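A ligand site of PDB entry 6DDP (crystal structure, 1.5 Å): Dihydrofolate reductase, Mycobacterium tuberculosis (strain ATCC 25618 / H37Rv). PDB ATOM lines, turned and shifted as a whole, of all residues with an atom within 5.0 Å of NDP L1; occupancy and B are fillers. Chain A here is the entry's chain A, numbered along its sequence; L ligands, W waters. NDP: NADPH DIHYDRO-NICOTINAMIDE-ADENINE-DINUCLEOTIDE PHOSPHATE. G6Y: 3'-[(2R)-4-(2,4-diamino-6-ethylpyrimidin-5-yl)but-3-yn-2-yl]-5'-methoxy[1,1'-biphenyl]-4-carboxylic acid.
O of Leu 65 lies close to O4B of NDP L1 (3.5 Å). Residues that only touch NDP L1: Ile 94 (3.1 Å), Gly 43 (3.2 Å), Gly 18 (3.4 Å), Gly 80 (3.4 Å), Tyr 100 (3.4 Å), Trp 6 (3.4 Å), Gly 15 (3.5 Å), Gly 95 (3.6 Å), Ala 126 (3.7 Å), Ile 20 (3.7 Å), Leu 102 (3.7 Å) and Arg 16 (3.8 Å). Within 4 Å of NDP L1: Trp 6, Ala 7, Ile 14, Gly 15, Arg 16, Gly 18, Asp 19, Ile 20, Gly 43, Arg 44, Arg 45, Thr 46, Leu 65, Ser 66, Arg 67, Gln 68, Gly 80, Ile 94, Gly 95, Gly 96, Gly 97, Gln 98, Val 99, Tyr 100, Leu 102 and Ala 126. The nearest printed residue that does not touch NDP L1 is Ser 49 (4.1 Å).
Water W1 lies within hydrogen-bond range of O3D of NDP L1, N of Gly 18 and N of Gly 17. Water W3 bridges OG of Ser 49 (2.7 Å) and O2D of NDP L1 (2.8 Å). Water W2 bridges O3X of NDP L1 and NH1 of Arg 67.
An oxygen (O3X) of NDP L1 sits at hydrogen-bond distance from the backbone NH (N) of Arg 67, 2.7 Å away. O of Ala 7 sits at hydrogen-bond distance from N7N of NDP L1 (2.8 Å). NH1 of Arg 45 is in salt-bridge range of O1N of NDP L1, 3.1 Å away. O5B of NDP L1 lies within hydrogen-bond range of N of Arg 44. The backbone NH (N) of Val 99 is in hydrogen-bond range of an oxygen (O1A) of NDP L1 (3.3 Å). The backbone carbonyl oxygen (O) of Asp 19 is in hydrogen-bond range of an oxygen (O3D) of NDP L1, at 3.5 Å. An oxygen (O2A) of NDP L1 is in hydrogen-bond range of the side-chain hydroxyl (OG1) of Thr 46. O of Ile 94 lies within hydrogen-bond range of NAH of G6Y L2 (3.0 Å). O7N of NDP L1 lies within hydrogen-bond range of N of Ala 7 (2.9 Å). The backbone carbonyl oxygen (O) of Ile 14 is in hydrogen-bond range of a nitrogen (N7N) of NDP L1, at 2.9 Å. The backbone NH (N) of Arg 45 is in hydrogen-bond range of an oxygen (O5B) of NDP L1 (3.4 Å). An oxygen (O2X) of NDP L1 is in salt-bridge range of the guanidinium group (NE) of Arg 44 (2.8 Å). N of Asp 19 sits at hydrogen-bond distance from O3D of NDP L1 (3.4 Å). The side-chain hydroxyl (OH) of Tyr 100 lies within hydrogen-bond range of a nitrogen (NAH) of G6Y L2, 3.3 Å away. The backbone NH (N) of Gly 96 is in hydrogen-bond range of an oxygen (O2A) of NDP L1. N of Thr 46 is in hydrogen-bond range of O2A of NDP L1, at 3.1 Å. A nitrogen (N3A) of NDP L1 lies close to the backbone NH (N) of Ser 66. An oxygen (O2N) of NDP L1 is in hydrogen-bond range of the backbone NH (N) of Gln 98 (2.8 Å). The backbone NH of Gly 97 sits at hydrogen-bond distance from an oxygen (O2N) of NDP L1 (2.9 Å). NE2 of Gln 68 sits at hydrogen-bond distance from O2X of NDP L1, at 2.6 Å. The side-chain hydroxyl of Ser 66 is in hydrogen-bond range of an oxygen (O2X) of NDP L1, at 2.7 Å. NAH of G6Y L2 is in hydrogen-bond range of O of Ile 5 (2.9 Å).
The backbone NH of Gly 95 sits at hydrogen-bond distance from the side-chain hydroxyl of Tyr 100 (3.4 Å). The backbone NH (N) of Gln 68 lies within hydrogen-bond range of the side-chain hydroxyl (OG) of Ser 66. O of Gly 15 sits at hydrogen-bond distance from N of Ala 126, 2.9 Å away. NH1 of Arg 45 lies close to NE2 of Gln 98, 3.3 Å away. The backbone carbonyl oxygen (O) of Ala 126 sits at hydrogen-bond distance from the backbone NH (N) of Ile 14 (2.9 Å). OG1 of Thr 46 is in hydrogen-bond range of N of Gly 96 (3.0 Å). O of Ile 5 is in hydrogen-bond range of OH of Tyr 100 (2.7 Å). The backbone carbonyl oxygen (O) of Ile 94 is in hydrogen-bond range of the side-chain hydroxyl (OH) of Tyr 100 (3.1 Å).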
ATOM      1  N   ILE A   5     -17.002  17.379   0.677  1.00  0.00           N
ATOM      2  CA  ILE A   5     -17.409  18.108  -0.518  1.00  0.00           C
ATOM      3  C   ILE A   5     -17.065  19.581  -0.322  1.00  0.00           C
ATOM      4  O   ILE A   5     -17.364  20.159   0.716  1.00  0.00           O
ATOM      5  CB  ILE A   5     -18.908  17.895  -0.834  1.00  0.00           C
ATOM      6  CG1 ILE A   5     -19.303  18.668  -2.094  1.00  0.00           C
ATOM      7  CG2 ILE A   5     -19.791  18.258   0.371  1.00  0.00           C
ATOM      8  CD1 ILE A   5     -20.656  18.225  -2.670  1.00  0.00           C
ATOM      9  N   TRP A   6     -16.390  20.171  -1.304  1.00  0.00           N
ATOM     10  CA  TRP A   6     -16.054  21.589  -1.227  1.00  0.00           C
ATOM     11  C   TRP A   6     -15.920  22.192  -2.606  1.00  0.00           C
ATOM     12  O   TRP A   6     -15.771  21.482  -3.592  1.00  0.00           O
ATOM     13  CB  TRP A   6     -14.750  21.822  -0.456  1.00  0.00           C
ATOM     14  CG  TRP A   6     -13.456  21.411  -1.144  1.00  0.00           C
ATOM     15  CD1 TRP A   6     -12.726  22.150  -2.038  1.00  0.00           C
ATOM     16  CD2 TRP A   6     -12.719  20.198  -0.939  1.00  0.00           C
ATOM     17  NE1 TRP A   6     -11.596  21.454  -2.411  1.00  0.00           N
ATOM     18  CE2 TRP A   6     -11.569  20.263  -1.751  1.00  0.00           C
ATOM     19  CE3 TRP A   6     -12.939  19.055  -0.146  1.00  0.00           C
ATOM     20  CZ2 TRP A   6     -10.622  19.222  -1.799  1.00  0.00           C
ATOM     21  CZ3 TRP A   6     -11.996  18.021  -0.202  1.00  0.00           C
ATOM     22  CH2 TRP A   6     -10.846  18.116  -1.014  1.00  0.00           C
ATOM     23  N   ALA A   7     -15.967  23.528  -2.650  1.00  0.00           N
ATOM     24  CA  ALA A   7     -15.632  24.280  -3.842  1.00  0.00           C
ATOM     25  C   ALA A   7     -14.427  25.131  -3.538  1.00  0.00           C
ATOM     26  O   ALA A   7     -14.395  25.819  -2.518  1.00  0.00           O
ATOM     27  CB  ALA A   7     -16.809  25.149  -4.276  1.00  0.00           C
ATOM     28  N   ILE A  14     -10.967  28.413  -0.101  1.00  0.00           N
ATOM     29  CA  ILE A  14     -12.383  28.067  -0.002  1.00  0.00           C
ATOM     30  C   ILE A  14     -13.195  29.112   0.769  1.00  0.00           C
ATOM     31  O   ILE A  14     -14.423  29.126   0.727  1.00  0.00           O
ATOM     32  CB  ILE A  14     -12.609  26.697   0.680  1.00  0.00           C
ATOM     33  CG1 ILE A  14     -12.145  26.703   2.142  1.00  0.00           C
ATOM     34  CG2 ILE A  14     -11.937  25.591  -0.118  1.00  0.00           C
ATOM     35  CD1 ILE A  14     -12.549  25.447   2.889  1.00  0.00           C
ATOM     36  N   GLY A  15     -12.500  29.985   1.490  1.00  0.00           N
ATOM     37  CA  GLY A  15     -13.169  30.948   2.339  1.00  0.00           C
ATOM     38  C   GLY A  15     -12.285  32.123   2.721  1.00  0.00           C
ATOM     39  O   GLY A  15     -11.073  31.966   2.864  1.00  0.00           O
ATOM     40  N   ARG A  16     -12.889  33.291   2.864  1.00  0.00           N
ATOM     41  CA  ARG A  16     -12.168  34.480   3.298  1.00  0.00           C
ATOM     42  C   ARG A  16     -13.161  35.397   3.994  1.00  0.00           C
ATOM     43  O   ARG A  16     -14.257  35.617   3.491  1.00  0.00           O
ATOM     44  CB  ARG A  16     -11.497  35.192   2.116  1.00  0.00           C
ATOM     45  CG  ARG A  16     -10.735  36.458   2.476  1.00  0.00           C
ATOM     46  CD  ARG A  16     -10.008  37.018   1.258  1.00  0.00           C
ATOM     47  NE  ARG A  16      -8.986  36.109   0.772  1.00  0.00           N
ATOM     48  CZ  ARG A  16      -8.404  36.176  -0.420  1.00  0.00           C
ATOM     49  NH1 ARG A  16      -8.766  37.123  -1.273  1.00  0.00           N
ATOM     50  NH2 ARG A  16      -7.478  35.289  -0.760  1.00  0.00           N
ATOM     51  N   GLY A  17     -12.807  35.910   5.175  1.00  0.00           N
ATOM     52  CA  GLY A  17     -13.684  36.810   5.894  1.00  0.00           C
ATOM     53  C   GLY A  17     -15.031  36.178   6.253  1.00  0.00           C
ATOM     54  O   GLY A  17     -16.045  36.867   6.358  1.00  0.00           O
ATOM     55  N   GLY A  18     -15.027  34.862   6.434  1.00  0.00           N
ATOM     56  CA  GLY A  18     -16.225  34.156   6.850  1.00  0.00           C
ATOM     57  C   GLY A  18     -17.233  33.911   5.744  1.00  0.00           C
ATOM     58  O   GLY A  18     -18.359  33.475   6.012  1.00  0.00           O
ATOM     59  N   ASP A  19     -16.846  34.177   4.503  1.00  0.00           N
ATOM     60  CA  ASP A  19     -17.740  33.966   3.370  1.00  0.00           C
ATOM     61  C   ASP A  19     -16.996  33.194   2.267  1.00  0.00           C
ATOM     62  O   ASP A  19     -15.769  33.067   2.303  1.00  0.00           O
ATOM     63  CB  ASP A  19     -18.261  35.295   2.827  1.00  0.00           C
ATOM     64  CG  ASP A  19     -19.462  35.133   1.893  1.00  0.00           C
ATOM     65  OD1 ASP A  19     -19.611  34.072   1.244  1.00  0.00           O
ATOM     66  OD2 ASP A  19     -20.250  36.099   1.778  1.00  0.00           O
ATOM     67  N   ILE A  20     -17.754  32.678   1.306  1.00  0.00           N
ATOM     68  CA  ILE A  20     -17.177  32.078   0.105  1.00  0.00           C
ATOM     69  C   ILE A  20     -17.007  33.174  -0.925  1.00  0.00           C
ATOM     70  O   ILE A  20     -17.973  33.835  -1.298  1.00  0.00           O
ATOM     71  CB  ILE A  20     -18.078  30.951  -0.440  1.00  0.00           C
ATOM     72  CG1 ILE A  20     -18.236  29.852   0.611  1.00  0.00           C
ATOM     73  CG2 ILE A  20     -17.504  30.374  -1.733  1.00  0.00           C
ATOM     74  CD1 ILE A  20     -19.130  28.696   0.165  1.00  0.00           C
ATOM     75  N   TRP A  22     -16.940  33.847  -3.987  1.00  0.00           N
ATOM     76  CA  TRP A  22     -17.514  33.866  -5.323  1.00  0.00           C
ATOM     77  C   TRP A  22     -18.964  33.432  -5.278  1.00  0.00           C
ATOM     78  O   TRP A  22     -19.457  32.932  -4.257  1.00  0.00           O
ATOM     79  CB  TRP A  22     -16.737  32.968  -6.284  1.00  0.00           C
ATOM     80  CG  TRP A  22     -16.703  31.562  -5.800  1.00  0.00           C
ATOM     81  CD1 TRP A  22     -17.680  30.614  -5.932  1.00  0.00           C
ATOM     82  CD2 TRP A  22     -15.647  30.946  -5.051  1.00  0.00           C
ATOM     83  NE1 TRP A  22     -17.290  29.446  -5.313  1.00  0.00           N
ATOM     84  CE2 TRP A  22     -16.045  29.630  -4.778  1.00  0.00           C
ATOM     85  CE3 TRP A  22     -14.404  31.379  -4.582  1.00  0.00           C
ATOM     86  CZ2 TRP A  22     -15.243  28.745  -4.063  1.00  0.00           C
ATOM     87  CZ3 TRP A  22     -13.605  30.501  -3.887  1.00  0.00           C
ATOM     88  CH2 TRP A  22     -14.032  29.203  -3.628  1.00  0.00           C
ATOM     89  N   GLY A  43     -18.208  22.566  10.669  1.00  0.00           N
ATOM     90  CA  GLY A  43     -17.721  23.341  11.798  1.00  0.00           C
ATOM     91  C   GLY A  43     -18.661  24.471  12.171  1.00  0.00           C
ATOM     92  O   GLY A  43     -19.451  24.938  11.345  1.00  0.00           O
ATOM     93  N   ARG A  44     -18.585  24.908  13.424  1.00  0.00           N
ATOM     94  CA  ARG A  44     -19.471  25.966  13.908  1.00  0.00           C
ATOM     95  C   ARG A  44     -19.382  27.249  13.071  1.00  0.00           C
ATOM     96  O   ARG A  44     -20.399  27.896  12.836  1.00  0.00           O
ATOM     97  CB  ARG A  44     -19.172  26.243  15.391  1.00  0.00           C
ATOM     98  CG  ARG A  44     -20.159  27.201  16.066  1.00  0.00           C
ATOM     99  CD  ARG A  44     -19.729  28.656  15.967  1.00  0.00           C
ATOM    100  NE  ARG A  44     -18.391  28.875  16.496  1.00  0.00           N
ATOM    101  CZ  ARG A  44     -17.681  29.976  16.322  1.00  0.00           C
ATOM    102  NH1 ARG A  44     -18.186  30.980  15.612  1.00  0.00           N
ATOM    103  NH2 ARG A  44     -16.475  30.091  16.853  1.00  0.00           N
ATOM    104  N   ARG A  45     -18.183  27.608  12.630  1.00  0.00           N
ATOM    105  CA  ARG A  45     -18.020  28.813  11.804  1.00  0.00           C
ATOM    106  C   ARG A  45     -18.779  28.701  10.478  1.00  0.00           C
ATOM    107  O   ARG A  45     -19.328  29.686   9.996  1.00  0.00           O
ATOM    108  CB  ARG A  45     -16.541  29.078  11.532  1.00  0.00           C
ATOM    109  CG  ARG A  45     -15.738  29.541  12.739  1.00  0.00           C
ATOM    110  CD  ARG A  45     -14.284  29.655  12.336  1.00  0.00           C
ATOM    111  NE  ARG A  45     -13.498  30.485  13.222  1.00  0.00           N
ATOM    112  CZ  ARG A  45     -12.177  30.652  13.094  1.00  0.00           C
ATOM    113  NH1 ARG A  45     -11.532  30.045  12.117  1.00  0.00           N
ATOM    114  NH2 ARG A  45     -11.525  31.432  13.946  1.00  0.00           N
ATOM    115  N   THR A  46     -18.818  27.499   9.909  1.00  0.00           N
ATOM    116  CA  THR A  46     -19.531  27.275   8.660  1.00  0.00           C
ATOM    117  C   THR A  46     -21.028  27.335   8.902  1.00  0.00           C
ATOM    118  O   THR A  46     -21.776  27.864   8.087  1.00  0.00           O
ATOM    119  CB  THR A  46     -19.126  25.939   8.041  1.00  0.00           C
ATOM    120  OG1 THR A  46     -17.766  26.040   7.579  1.00  0.00           O
ATOM    121  CG2 THR A  46     -20.021  25.585   6.873  1.00  0.00           C
ATOM    122  N   SER A  49     -22.042  30.875   8.919  1.00  0.00           N
ATOM    123  CA  SER A  49     -21.995  31.520   7.615  1.00  0.00           C
ATOM    124  C   SER A  49     -23.249  31.231   6.771  1.00  0.00           C
ATOM    125  O   SER A  49     -23.493  31.899   5.765  1.00  0.00           O
ATOM    126  CB  SER A  49     -20.762  31.087   6.832  1.00  0.00           C
ATOM    127  OG  SER A  49     -20.933  29.812   6.263  1.00  0.00           O
ATOM    128  N   LEU A  65     -20.098  20.847  14.656  1.00  0.00           N
ATOM    129  CA  LEU A  65     -19.019  20.593  15.592  1.00  0.00           C
ATOM    130  C   LEU A  65     -18.617  21.877  16.318  1.00  0.00           C
ATOM    131  O   LEU A  65     -18.317  22.889  15.685  1.00  0.00           O
ATOM    132  CB  LEU A  65     -17.828  19.993  14.840  1.00  0.00           C
ATOM    133  CG  LEU A  65     -16.726  19.288  15.617  1.00  0.00           C
ATOM    134  CD1 LEU A  65     -17.304  18.199  16.506  1.00  0.00           C
ATOM    135  CD2 LEU A  65     -15.708  18.716  14.661  1.00  0.00           C
ATOM    136  N   SER A  66     -18.624  21.836  17.643  1.00  0.00           N
ATOM    137  CA  SER A  66     -18.217  22.978  18.462  1.00  0.00           C
ATOM    138  C   SER A  66     -17.570  22.444  19.728  1.00  0.00           C
ATOM    139  O   SER A  66     -17.961  21.399  20.225  1.00  0.00           O
ATOM    140  CB  SER A  66     -19.421  23.865  18.802  1.00  0.00           C
ATOM    141  OG  SER A  66     -19.048  24.956  19.630  1.00  0.00           O
ATOM    142  N   ARG A  67     -16.572  23.138  20.243  1.00  0.00           N
ATOM    143  CA  ARG A  67     -15.994  22.729  21.512  1.00  0.00           C
ATOM    144  C   ARG A  67     -16.778  23.358  22.639  1.00  0.00           C
ATOM    145  O   ARG A  67     -16.584  23.047  23.828  1.00  0.00           O
ATOM    146  CB  ARG A  67     -14.527  23.108  21.594  1.00  0.00           C
ATOM    147  CG  ARG A  67     -13.633  22.138  20.889  1.00  0.00           C
ATOM    148  CD  ARG A  67     -12.177  22.418  21.242  1.00  0.00           C
ATOM    149  NE  ARG A  67     -11.268  21.667  20.379  1.00  0.00           N
ATOM    150  CZ  ARG A  67     -10.798  22.122  19.224  1.00  0.00           C
ATOM    151  NH1 ARG A  67     -11.160  23.328  18.787  1.00  0.00           N
ATOM    152  NH2 ARG A  67      -9.969  21.378  18.500  1.00  0.00           N
ATOM    153  N   GLN A  68     -17.660  24.277  22.260  1.00  0.00           N
ATOM    154  CA  GLN A  68     -18.556  24.918  23.201  1.00  0.00           C
ATOM    155  C   GLN A  68     -19.669  23.951  23.565  1.00  0.00           C
ATOM    156  O   GLN A  68     -20.549  23.666  22.743  1.00  0.00           O
ATOM    157  CB  GLN A  68     -19.167  26.198  22.635  1.00  0.00           C
ATOM    158  CG  GLN A  68     -18.242  27.085  21.814  1.00  0.00           C
ATOM    159  CD  GLN A  68     -18.969  28.307  21.269  1.00  0.00           C
ATOM    160  OE1 GLN A  68     -19.808  28.874  21.960  1.00  0.00           O
ATOM    161  NE2 GLN A  68     -18.636  28.718  20.044  1.00  0.00           N
ATOM    162  N   GLY A  80     -19.547  17.725  20.275  1.00  0.00           N
ATOM    163  CA  GLY A  80     -18.264  18.248  20.727  1.00  0.00           C
ATOM    164  C   GLY A  80     -17.048  17.480  20.251  1.00  0.00           C
ATOM    165  O   GLY A  80     -15.915  17.843  20.571  1.00  0.00           O
ATOM    166  N   SER A  81     -17.264  16.410  19.492  1.00  0.00           N
ATOM    167  CA  SER A  81     -16.145  15.636  18.965  1.00  0.00           C
ATOM    168  C   SER A  81     -16.451  15.023  17.599  1.00  0.00           C
ATOM    169  O   SER A  81     -17.623  14.790  17.259  1.00  0.00           O
ATOM    170  CB  SER A  81     -15.771  14.534  19.953  1.00  0.00           C
ATOM    171  OG  SER A  81     -16.800  13.556  20.015  1.00  0.00           O
ATOM    172  N   ILE A  94     -19.048  19.187   5.005  1.00  0.00           N
ATOM    173  CA  ILE A  94     -19.311  20.285   4.082  1.00  0.00           C
ATOM    174  C   ILE A  94     -18.564  21.567   4.464  1.00  0.00           C
ATOM    175  O   ILE A  94     -18.830  22.645   3.910  1.00  0.00           O
ATOM    176  CB  ILE A  94     -20.841  20.586   4.005  1.00  0.00           C
ATOM    177  CG1 ILE A  94     -21.376  21.147   5.324  1.00  0.00           C
ATOM    178  CG2 ILE A  94     -21.577  19.347   3.544  1.00  0.00           C
ATOM    179  CD1 ILE A  94     -22.760  21.791   5.208  1.00  0.00           C
ATOM    180  N   GLY A  95     -17.611  21.447   5.378  1.00  0.00           N
ATOM    181  CA  GLY A  95     -16.746  22.578   5.698  1.00  0.00           C
ATOM    182  C   GLY A  95     -16.641  22.857   7.177  1.00  0.00           C
ATOM    183  O   GLY A  95     -17.356  22.261   7.971  1.00  0.00           O
ATOM    184  N   GLY A  96     -15.753  23.769   7.569  1.00  0.00           N
ATOM    185  CA  GLY A  96     -14.884  24.507   6.660  1.00  0.00           C
ATOM    186  C   GLY A  96     -13.451  23.981   6.723  1.00  0.00           C
ATOM    187  O   GLY A  96     -13.230  22.786   6.828  1.00  0.00           O
ATOM    188  N   GLY A  97     -12.483  24.891   6.636  1.00  0.00           N
ATOM    189  CA  GLY A  97     -11.084  24.497   6.594  1.00  0.00           C
ATOM    190  C   GLY A  97     -10.640  23.601   7.718  1.00  0.00           C
ATOM    191  O   GLY A  97     -10.018  22.568   7.481  1.00  0.00           O
ATOM    192  N   GLN A  98     -10.958  23.973   8.957  1.00  0.00           N
ATOM    193  CA  GLN A  98     -10.552  23.183  10.110  1.00  0.00           C
ATOM    194  C   GLN A  98     -11.157  21.799  10.047  1.00  0.00           C
ATOM    195  O   GLN A  98     -10.479  20.805  10.296  1.00  0.00           O
ATOM    196  CB  GLN A  98     -10.964  23.843  11.415  1.00  0.00           C
ATOM    197  CG  GLN A  98     -10.302  25.193  11.695  1.00  0.00           C
ATOM    198  CD  GLN A  98     -10.697  25.731  13.050  1.00  0.00           C
ATOM    199  OE1 GLN A  98     -11.012  24.974  13.972  1.00  0.00           O
ATOM    200  NE2 GLN A  98     -10.706  27.049  13.174  1.00  0.00           N
ATOM    201  N   VAL A  99     -12.443  21.726   9.719  1.00  0.00           N
ATOM    202  CA  VAL A  99     -13.122  20.449   9.815  1.00  0.00           C
ATOM    203  C   VAL A  99     -12.773  19.521   8.643  1.00  0.00           C
ATOM    204  O   VAL A  99     -12.703  18.314   8.841  1.00  0.00           O
ATOM    205  CB  VAL A  99     -14.636  20.678   9.936  1.00  0.00           C
ATOM    206  CG1 VAL A  99     -15.409  19.368   9.853  1.00  0.00           C
ATOM    207  CG2 VAL A  99     -14.906  21.362  11.262  1.00  0.00           C
ATOM    208  N   TYR A 100     -12.510  20.065   7.456  1.00  0.00           N
ATOM    209  CA  TYR A 100     -11.965  19.225   6.372  1.00  0.00           C
ATOM    210  C   TYR A 100     -10.674  18.565   6.812  1.00  0.00           C
ATOM    211  O   TYR A 100     -10.468  17.384   6.549  1.00  0.00           O
ATOM    212  CB  TYR A 100     -11.685  20.026   5.105  1.00  0.00           C
ATOM    213  CG  TYR A 100     -12.915  20.508   4.358  1.00  0.00           C
ATOM    214  CD1 TYR A 100     -14.007  19.683   4.133  1.00  0.00           C
ATOM    215  CD2 TYR A 100     -12.981  21.804   3.884  1.00  0.00           C
ATOM    216  CE1 TYR A 100     -15.130  20.145   3.438  1.00  0.00           C
ATOM    217  CE2 TYR A 100     -14.094  22.269   3.202  1.00  0.00           C
ATOM    218  CZ  TYR A 100     -15.164  21.445   2.997  1.00  0.00           C
ATOM    219  OH  TYR A 100     -16.244  21.967   2.327  1.00  0.00           O
ATOM    220  N   LEU A 102      -9.638  17.922   9.893  1.00  0.00           N
ATOM    221  CA  LEU A 102      -9.974  16.953  10.938  1.00  0.00           C
ATOM    222  C   LEU A 102     -10.570  15.669  10.364  1.00  0.00           C
ATOM    223  O   LEU A 102     -10.270  14.575  10.832  1.00  0.00           O
ATOM    224  CB  LEU A 102     -10.978  17.575  11.921  1.00  0.00           C
ATOM    225  CG  LEU A 102     -11.329  16.793  13.178  1.00  0.00           C
ATOM    226  CD1 LEU A 102     -10.122  16.739  14.106  1.00  0.00           C
ATOM    227  CD2 LEU A 102     -12.514  17.427  13.873  1.00  0.00           C
ATOM    228  N   ALA A 126      -9.413  30.333   4.673  1.00  0.00           N
ATOM    229  CA  ALA A 126      -9.756  28.933   4.788  1.00  0.00           C
ATOM    230  C   ALA A 126      -9.338  28.259   3.497  1.00  0.00           C
ATOM    231  O   ALA A 126      -9.610  28.789   2.402  1.00  0.00           O
ATOM    232  CB  ALA A 126     -11.232  28.744   5.059  1.00  0.00           C
HETATM  233  PA  NDP L   1     -14.936  25.714  10.434  1.00  0.00           P
HETATM  234  O1A NDP L   1     -14.141  24.528  10.126  1.00  0.00           O
HETATM  235  O2A NDP L   1     -16.161  26.002   9.619  1.00  0.00           O
HETATM  236  O5B NDP L   1     -15.497  25.643  11.973  1.00  0.00           O
HETATM  237  C5B NDP L   1     -14.409  25.755  12.863  1.00  0.00           C
HETATM  238  C4B NDP L   1     -15.028  25.475  14.258  1.00  0.00           C
HETATM  239  O4B NDP L   1     -15.307  24.107  14.390  1.00  0.00           O
HETATM  240  C3B NDP L   1     -14.126  25.870  15.446  1.00  0.00           C
HETATM  241  O3B NDP L   1     -14.196  27.230  15.708  1.00  0.00           O
HETATM  242  C2B NDP L   1     -14.879  25.082  16.562  1.00  0.00           C
HETATM  243  O2B NDP L   1     -16.071  25.589  16.840  1.00  0.00           O
HETATM  244  C1B NDP L   1     -15.204  23.759  15.783  1.00  0.00           C
HETATM  245  N9A NDP L   1     -14.183  22.744  15.900  1.00  0.00           N
HETATM  246  C8A NDP L   1     -12.968  22.651  15.185  1.00  0.00           C
HETATM  247  N7A NDP L   1     -12.231  21.572  15.530  1.00  0.00           N
HETATM  248  C5A NDP L   1     -13.011  20.949  16.511  1.00  0.00           C
HETATM  249  C6A NDP L   1     -12.809  19.785  17.254  1.00  0.00           C
HETATM  250  N6A NDP L   1     -11.660  19.041  17.072  1.00  0.00           N
HETATM  251  N1A NDP L   1     -13.722  19.363  18.162  1.00  0.00           N
HETATM  252  C2A NDP L   1     -14.839  20.157  18.293  1.00  0.00           C
HETATM  253  N3A NDP L   1     -15.194  21.285  17.651  1.00  0.00           N
HETATM  254  C4A NDP L   1     -14.234  21.672  16.747  1.00  0.00           C
HETATM  255  O3  NDP L   1     -13.971  27.111  10.520  1.00  0.00           O
HETATM  256  PN  NDP L   1     -13.038  27.546   9.271  1.00  0.00           P
HETATM  257  O1N NDP L   1     -12.775  28.980   9.493  1.00  0.00           O
HETATM  258  O2N NDP L   1     -11.924  26.586   8.944  1.00  0.00           O
HETATM  259  O5D NDP L   1     -13.991  27.498   7.799  1.00  0.00           O
HETATM  260  C5D NDP L   1     -14.857  28.586   7.687  1.00  0.00           C
HETATM  261  C4D NDP L   1     -14.647  29.211   6.283  1.00  0.00           C
HETATM  262  O4D NDP L   1     -14.837  28.199   5.253  1.00  0.00           O
HETATM  263  C3D NDP L   1     -15.696  30.330   5.989  1.00  0.00           C
HETATM  264  O3D NDP L   1     -15.050  31.346   5.260  1.00  0.00           O
HETATM  265  C2D NDP L   1     -16.701  29.599   5.100  1.00  0.00           C
HETATM  266  O2D NDP L   1     -17.377  30.466   4.229  1.00  0.00           O
HETATM  267  C1D NDP L   1     -15.737  28.710   4.270  1.00  0.00           C
HETATM  268  N1N NDP L   1     -16.431  27.564   3.651  1.00  0.00           N
HETATM  269  C2N NDP L   1     -16.240  27.282   2.304  1.00  0.00           C
HETATM  270  C3N NDP L   1     -16.741  26.147   1.760  1.00  0.00           C
HETATM  271  C7N NDP L   1     -16.502  25.876   0.361  1.00  0.00           C
HETATM  272  O7N NDP L   1     -16.753  24.790  -0.155  1.00  0.00           O
HETATM  273  N7N NDP L   1     -15.965  26.888  -0.412  1.00  0.00           N
HETATM  274  C4N NDP L   1     -17.486  25.147   2.544  1.00  0.00           C
HETATM  275  C5N NDP L   1     -17.719  25.572   3.926  1.00  0.00           C
HETATM  276  C6N NDP L   1     -17.229  26.703   4.429  1.00  0.00           C
HETATM  277  P2B NDP L   1     -16.157  26.551  18.366  1.00  0.00           P
HETATM  278  O1X NDP L   1     -15.165  27.603  17.944  1.00  0.00           O
HETATM  279  O2X NDP L   1     -17.634  26.954  18.405  1.00  0.00           O
HETATM  280  O3X NDP L   1     -15.689  25.514  19.348  1.00  0.00           O
HETATM  281  C4  G6Y L   2     -20.560  24.663  -1.532  1.00  0.00           C
HETATM  282  C5  G6Y L   2     -20.266  24.125  -0.282  1.00  0.00           C
HETATM  283  C6  G6Y L   2     -19.574  22.919  -0.252  1.00  0.00           C
HETATM  284  N1  G6Y L   2     -19.229  22.292  -1.384  1.00  0.00           N
HETATM  285  N3  G6Y L   2     -20.192  24.006  -2.629  1.00  0.00           N
HETATM  286  CBE G6Y L   2     -22.645  25.655  -2.251  1.00  0.00           C
HETATM  287  CBD G6Y L   2     -21.245  25.888  -1.675  1.00  0.00           C
HETATM  288  C2  G6Y L   2     -19.550  22.827  -2.568  1.00  0.00           C
HETATM  289  NAG G6Y L   2     -19.209  22.182  -3.686  1.00  0.00           N
HETATM  290  NAH G6Y L   2     -19.263  22.388   0.940  1.00  0.00           N
HETATM  291  CAI G6Y L   2     -20.659  24.832   0.901  1.00  0.00           C
HETATM  292  CAJ G6Y L   2     -21.017  25.488   1.793  1.00  0.00           C
HETATM  293  CAK G6Y L   2     -21.548  26.394   2.833  1.00  0.00           C
HETATM  294  CBC G6Y L   2     -22.038  25.575   4.041  1.00  0.00           C
HETATM  295  CAL G6Y L   2     -22.646  27.127   2.297  1.00  0.00           C
HETATM  296  CAM G6Y L   2     -23.775  26.489   1.732  1.00  0.00           C
HETATM  297  CAQ G6Y L   2     -22.627  28.525   2.313  1.00  0.00           C
HETATM  298  CAP G6Y L   2     -23.689  29.249   1.797  1.00  0.00           C
HETATM  299  OAX G6Y L   2     -23.628  30.624   1.832  1.00  0.00           O
HETATM  300  CAY G6Y L   2     -24.653  31.237   1.038  1.00  0.00           C
HETATM  301  CAO G6Y L   2     -24.794  28.605   1.244  1.00  0.00           C
HETATM  302  CAN G6Y L   2     -24.842  27.220   1.180  1.00  0.00           C
HETATM  303  CAR G6Y L   2     -25.970  26.559   0.651  1.00  0.00           C
HETATM  304  CAS G6Y L   2     -25.884  25.244   0.211  1.00  0.00           C
HETATM  305  CAT G6Y L   2     -27.001  24.557  -0.291  1.00  0.00           C
HETATM  306  CAU G6Y L   2     -28.241  25.194  -0.358  1.00  0.00           C
HETATM  307  CAZ G6Y L   2     -29.346  24.504  -0.854  1.00  0.00           C
HETATM  308  OBB G6Y L   2     -29.353  23.246  -0.857  1.00  0.00           O
HETATM  309  OBA G6Y L   2     -30.360  25.116  -1.265  1.00  0.00           O
HETATM  310  CAV G6Y L   2     -28.340  26.512   0.075  1.00  0.00           C
HETATM  311  CAW G6Y L   2     -27.219  27.192   0.584  1.00  0.00           C
HETATM  312  O   HOH W   1     -13.142  32.717   6.338  1.00  0.00           O
HETATM  313  O   HOH W   2     -12.816  25.557  19.713  1.00  0.00           O
HETATM  314  O   HOH W   3     -19.888  29.320   3.840  1.00  0.00           O
HETATM  315  O   HOH W   4      -9.478  27.614   8.317  1.00  0.00           O
